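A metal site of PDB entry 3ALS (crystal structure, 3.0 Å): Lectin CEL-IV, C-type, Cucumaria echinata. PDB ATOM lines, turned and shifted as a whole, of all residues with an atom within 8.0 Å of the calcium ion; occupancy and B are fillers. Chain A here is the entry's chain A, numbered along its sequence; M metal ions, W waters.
The side-chain carboxylate (OD2) of Asp 136 is in hydrogen-bond range of the side-chain hydroxyl (OG) of Ser 120, 2.6 Å away.
The backbone carbonyl oxygen (O) of Gly 112 lies close to the side-chain amide nitrogen (ND2) of Asn 115, at 3.3 Å.
The nearest printed residue that does not touch the calcium ion is Ala 135 (4.7 Å).
The calcium ion is bound by OD1 of Asn 116, 2.2 Å away.
The side-chain carboxylate (OE2) of Glu 113 is bound to the calcium ion (2.2 Å).
The backbone carbonyl oxygen (O) of Asp 136 binds the calcium ion, at 2.5 Å.
The side-chain carboxylate (OD1) of Asp 136 is bound to the calcium ion, 2.5 Å away.
Water W1 binds the calcium ion (2.5 Å).
The calcium ion is bound by the side-chain amide oxygen (OD1) of Asn 115.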
ATOM      1  N   TRP A  79       1.908 -24.145  34.273  1.00  0.00           N
ATOM      2  CA  TRP A  79       0.962 -25.187  33.882  1.00  0.00           C
ATOM      3  C   TRP A  79       1.683 -26.520  33.709  1.00  0.00           C
ATOM      4  O   TRP A  79       1.200 -27.565  34.076  1.00  0.00           O
ATOM      5  CB  TRP A  79       0.233 -24.821  32.548  1.00  0.00           C
ATOM      6  CG  TRP A  79      -0.654 -23.644  32.679  1.00  0.00           C
ATOM      7  CD1 TRP A  79      -0.248 -22.386  32.884  1.00  0.00           C
ATOM      8  CD2 TRP A  79      -2.115 -23.606  32.692  1.00  0.00           C
ATOM      9  NE1 TRP A  79      -1.337 -21.531  33.022  1.00  0.00           N
ATOM     10  CE2 TRP A  79      -2.497 -22.261  32.908  1.00  0.00           C
ATOM     11  CE3 TRP A  79      -3.116 -24.566  32.564  1.00  0.00           C
ATOM     12  CZ2 TRP A  79      -3.825 -21.847  33.000  1.00  0.00           C
ATOM     13  CZ3 TRP A  79      -4.462 -24.142  32.630  1.00  0.00           C
ATOM     14  CH2 TRP A  79      -4.791 -22.796  32.837  1.00  0.00           C
ATOM     15  N   GLN A  82       2.083 -30.820  30.981  1.00  0.00           N
ATOM     16  CA  GLN A  82       0.765 -31.211  30.608  1.00  0.00           C
ATOM     17  C   GLN A  82       0.743 -32.639  30.113  1.00  0.00           C
ATOM     18  O   GLN A  82       1.526 -33.006  29.209  1.00  0.00           O
ATOM     19  CB  GLN A  82       0.194 -30.257  29.575  1.00  0.00           C
ATOM     20  CG  GLN A  82      -0.200 -28.883  30.165  1.00  0.00           C
ATOM     21  CD  GLN A  82      -0.239 -27.845  29.061  1.00  0.00           C
ATOM     22  OE1 GLN A  82       0.708 -27.742  28.283  1.00  0.00           O
ATOM     23  NE2 GLN A  82      -1.321 -27.085  28.963  1.00  0.00           N
ATOM     24  N   TRP A 109     -11.831 -29.270  35.274  1.00  0.00           N
ATOM     25  CA  TRP A 109     -11.219 -28.101  34.647  1.00  0.00           C
ATOM     26  C   TRP A 109     -10.735 -27.102  35.671  1.00  0.00           C
ATOM     27  O   TRP A 109     -11.371 -26.885  36.714  1.00  0.00           O
ATOM     28  CB  TRP A 109     -12.177 -27.414  33.752  1.00  0.00           C
ATOM     29  CG  TRP A 109     -12.701 -28.258  32.732  1.00  0.00           C
ATOM     30  CD1 TRP A 109     -13.917 -28.814  32.727  1.00  0.00           C
ATOM     31  CD2 TRP A 109     -12.072 -28.622  31.508  1.00  0.00           C
ATOM     32  NE1 TRP A 109     -14.114 -29.536  31.556  1.00  0.00           N
ATOM     33  CE2 TRP A 109     -12.984 -29.449  30.798  1.00  0.00           C
ATOM     34  CE3 TRP A 109     -10.810 -28.366  30.939  1.00  0.00           C
ATOM     35  CZ2 TRP A 109     -12.705 -30.019  29.543  1.00  0.00           C
ATOM     36  CZ3 TRP A 109     -10.508 -28.913  29.673  1.00  0.00           C
ATOM     37  CH2 TRP A 109     -11.482 -29.733  28.988  1.00  0.00           C
ATOM     38  N   VAL A 110      -9.568 -26.527  35.356  1.00  0.00           N
ATOM     39  CA  VAL A 110      -9.070 -25.327  36.008  1.00  0.00           C
ATOM     40  C   VAL A 110     -10.037 -24.221  35.637  1.00  0.00           C
ATOM     41  O   VAL A 110     -10.515 -24.131  34.471  1.00  0.00           O
ATOM     42  CB  VAL A 110      -7.663 -24.876  35.489  1.00  0.00           C
ATOM     43  CG1 VAL A 110      -7.147 -23.644  36.284  1.00  0.00           C
ATOM     44  CG2 VAL A 110      -6.666 -25.985  35.570  1.00  0.00           C
ATOM     45  N   GLY A 112     -11.679 -21.148  34.288  1.00  0.00           N
ATOM     46  CA  GLY A 112     -11.469 -20.566  32.956  1.00  0.00           C
ATOM     47  C   GLY A 112     -11.430 -21.600  31.802  1.00  0.00           C
ATOM     48  O   GLY A 112     -11.495 -21.257  30.581  1.00  0.00           O
ATOM     49  N   GLU A 113     -11.315 -22.893  32.131  1.00  0.00           N
ATOM     50  CA  GLU A 113     -11.081 -23.893  31.079  1.00  0.00           C
ATOM     51  C   GLU A 113     -12.386 -24.678  30.937  1.00  0.00           C
ATOM     52  O   GLU A 113     -13.153 -24.724  31.873  1.00  0.00           O
ATOM     53  CB  GLU A 113      -9.845 -24.739  31.437  1.00  0.00           C
ATOM     54  CG  GLU A 113      -8.495 -23.933  31.705  1.00  0.00           C
ATOM     55  CD  GLU A 113      -7.786 -23.416  30.403  1.00  0.00           C
ATOM     56  OE1 GLU A 113      -7.163 -22.289  30.431  1.00  0.00           O
ATOM     57  OE2 GLU A 113      -7.893 -24.123  29.348  1.00  0.00           O
ATOM     58  N   PRO A 114     -12.706 -25.203  29.730  1.00  0.00           N
ATOM     59  CA  PRO A 114     -12.023 -25.045  28.436  1.00  0.00           C
ATOM     60  C   PRO A 114     -12.228 -23.644  27.908  1.00  0.00           C
ATOM     61  O   PRO A 114     -12.997 -22.870  28.504  1.00  0.00           O
ATOM     62  CB  PRO A 114     -12.744 -26.045  27.506  1.00  0.00           C
ATOM     63  CG  PRO A 114     -13.975 -26.432  28.178  1.00  0.00           C
ATOM     64  CD  PRO A 114     -13.968 -25.966  29.613  1.00  0.00           C
ATOM     65  N   ASN A 115     -11.546 -23.331  26.812  1.00  0.00           N
ATOM     66  CA  ASN A 115     -11.471 -21.991  26.256  1.00  0.00           C
ATOM     67  C   ASN A 115     -10.630 -21.939  24.951  1.00  0.00           C
ATOM     68  O   ASN A 115     -10.308 -20.883  24.454  1.00  0.00           O
ATOM     69  CB  ASN A 115     -10.940 -21.006  27.311  1.00  0.00           C
ATOM     70  CG  ASN A 115      -9.470 -21.087  27.484  1.00  0.00           C
ATOM     71  OD1 ASN A 115      -8.767 -21.668  26.662  1.00  0.00           O
ATOM     72  ND2 ASN A 115      -8.974 -20.497  28.548  1.00  0.00           N
ATOM     73  N   ASN A 116     -10.247 -23.072  24.388  1.00  0.00           N
ATOM     74  CA  ASN A 116      -9.616 -23.052  23.082  1.00  0.00           C
ATOM     75  C   ASN A 116     -10.425 -23.913  22.125  1.00  0.00           C
ATOM     76  O   ASN A 116      -9.845 -24.501  21.189  1.00  0.00           O
ATOM     77  CB  ASN A 116      -8.171 -23.554  23.157  1.00  0.00           C
ATOM     78  CG  ASN A 116      -7.263 -22.736  24.139  1.00  0.00           C
ATOM     79  OD1 ASN A 116      -7.000 -23.143  25.277  1.00  0.00           O
ATOM     80  ND2 ASN A 116      -6.742 -21.623  23.662  1.00  0.00           N
ATOM     81  N   GLY A 117     -11.746 -23.981  22.351  1.00  0.00           N
ATOM     82  CA  GLY A 117     -12.664 -24.760  21.492  1.00  0.00           C
ATOM     83  C   GLY A 117     -12.864 -24.015  20.204  1.00  0.00           C
ATOM     84  O   GLY A 117     -12.364 -22.904  20.074  1.00  0.00           O
ATOM     85  N   SER A 120     -10.892 -28.805  21.041  1.00  0.00           N
ATOM     86  CA  SER A 120      -9.740 -28.878  21.924  1.00  0.00           C
ATOM     87  C   SER A 120      -9.782 -30.211  22.668  1.00  0.00           C
ATOM     88  O   SER A 120     -10.747 -31.001  22.479  1.00  0.00           O
ATOM     89  CB  SER A 120      -9.699 -27.726  22.919  1.00  0.00           C
ATOM     90  OG  SER A 120     -10.942 -27.474  23.467  1.00  0.00           O
ATOM     91  N   ARG A 121      -8.739 -30.487  23.478  1.00  0.00           N
ATOM     92  CA  ARG A 121      -8.631 -31.757  24.186  1.00  0.00           C
ATOM     93  C   ARG A 121      -8.062 -31.461  25.564  1.00  0.00           C
ATOM     94  O   ARG A 121      -7.399 -30.439  25.750  1.00  0.00           O
ATOM     95  CB  ARG A 121      -7.729 -32.679  23.449  1.00  0.00           C
ATOM     96  CG  ARG A 121      -7.863 -32.571  21.981  1.00  0.00           C
ATOM     97  CD  ARG A 121      -8.635 -33.686  21.447  1.00  0.00           C
ATOM     98  NE  ARG A 121      -9.919 -33.274  20.961  1.00  0.00           N
ATOM     99  CZ  ARG A 121     -10.496 -33.515  19.774  1.00  0.00           C
ATOM    100  NH1 ARG A 121      -9.918 -34.218  18.794  1.00  0.00           N
ATOM    101  NH2 ARG A 121     -11.714 -33.003  19.609  1.00  0.00           N
ATOM    102  N   TRP A 134      -7.607 -29.624  34.881  1.00  0.00           N
ATOM    103  CA  TRP A 134      -7.442 -29.794  33.435  1.00  0.00           C
ATOM    104  C   TRP A 134      -7.298 -28.499  32.666  1.00  0.00           C
ATOM    105  O   TRP A 134      -7.817 -27.449  33.108  1.00  0.00           O
ATOM    106  CB  TRP A 134      -8.609 -30.573  32.836  1.00  0.00           C
ATOM    107  CG  TRP A 134      -9.005 -31.805  33.610  1.00  0.00           C
ATOM    108  CD1 TRP A 134      -8.201 -32.603  34.401  1.00  0.00           C
ATOM    109  CD2 TRP A 134     -10.302 -32.368  33.664  1.00  0.00           C
ATOM    110  NE1 TRP A 134      -8.939 -33.628  34.952  1.00  0.00           N
ATOM    111  CE2 TRP A 134     -10.222 -33.519  34.498  1.00  0.00           C
ATOM    112  CE3 TRP A 134     -11.524 -32.019  33.105  1.00  0.00           C
ATOM    113  CZ2 TRP A 134     -11.334 -34.321  34.766  1.00  0.00           C
ATOM    114  CZ3 TRP A 134     -12.607 -32.820  33.350  1.00  0.00           C
ATOM    115  CH2 TRP A 134     -12.512 -33.954  34.173  1.00  0.00           C
ATOM    116  N   ALA A 135      -6.616 -28.568  31.529  1.00  0.00           N
ATOM    117  CA  ALA A 135      -6.559 -27.453  30.590  1.00  0.00           C
ATOM    118  C   ALA A 135      -6.905 -28.003  29.255  1.00  0.00           C
ATOM    119  O   ALA A 135      -6.596 -29.158  28.972  1.00  0.00           O
ATOM    120  CB  ALA A 135      -5.179 -26.849  30.549  1.00  0.00           C
ATOM    121  N   ASP A 136      -7.553 -27.209  28.416  1.00  0.00           N
ATOM    122  CA  ASP A 136      -7.791 -27.661  27.033  1.00  0.00           C
ATOM    123  C   ASP A 136      -6.807 -26.996  26.071  1.00  0.00           C
ATOM    124  O   ASP A 136      -6.493 -25.804  26.207  1.00  0.00           O
ATOM    125  CB  ASP A 136      -9.221 -27.393  26.572  1.00  0.00           C
ATOM    126  CG  ASP A 136      -9.501 -25.880  26.271  1.00  0.00           C
ATOM    127  OD1 ASP A 136      -8.941 -24.928  26.951  1.00  0.00           O
ATOM    128  OD2 ASP A 136     -10.332 -25.724  25.337  1.00  0.00           O
ATOM    129  N   VAL A 137      -6.330 -27.788  25.127  1.00  0.00           N
ATOM    130  CA  VAL A 137      -5.188 -27.415  24.339  1.00  0.00           C
ATOM    131  C   VAL A 137      -5.560 -27.882  22.964  1.00  0.00           C
ATOM    132  O   VAL A 137      -6.629 -28.455  22.765  1.00  0.00           O
ATOM    133  CB  VAL A 137      -3.911 -28.127  24.816  1.00  0.00           C
ATOM    134  CG1 VAL A 137      -3.697 -27.963  26.322  1.00  0.00           C
ATOM    135  CG2 VAL A 137      -3.903 -29.607  24.411  1.00  0.00           C
ATOM    136  N   TYR A 138      -4.702 -27.641  21.986  1.00  0.00           N
ATOM    137  CA  TYR A 138      -5.111 -27.975  20.639  1.00  0.00           C
ATOM    138  C   TYR A 138      -4.694 -29.354  20.285  1.00  0.00           C
ATOM    139  O   TYR A 138      -3.599 -29.814  20.631  1.00  0.00           O
ATOM    140  CB  TYR A 138      -4.535 -27.048  19.589  1.00  0.00           C
ATOM    141  CG  TYR A 138      -5.057 -25.634  19.635  1.00  0.00           C
ATOM    142  CD1 TYR A 138      -4.948 -24.889  20.821  1.00  0.00           C
ATOM    143  CD2 TYR A 138      -5.604 -25.017  18.490  1.00  0.00           C
ATOM    144  CE1 TYR A 138      -5.393 -23.551  20.871  1.00  0.00           C
ATOM    145  CE2 TYR A 138      -6.054 -23.700  18.522  1.00  0.00           C
ATOM    146  CZ  TYR A 138      -5.955 -22.988  19.694  1.00  0.00           C
ATOM    147  OH  TYR A 138      -6.418 -21.715  19.703  1.00  0.00           O
HETATM  148 CA    CA M   1      -6.807 -23.652  27.435  1.00  0.00          CA
HETATM  149  O   HOH W   1      -4.627 -23.194  28.676  1.00  0.00           O
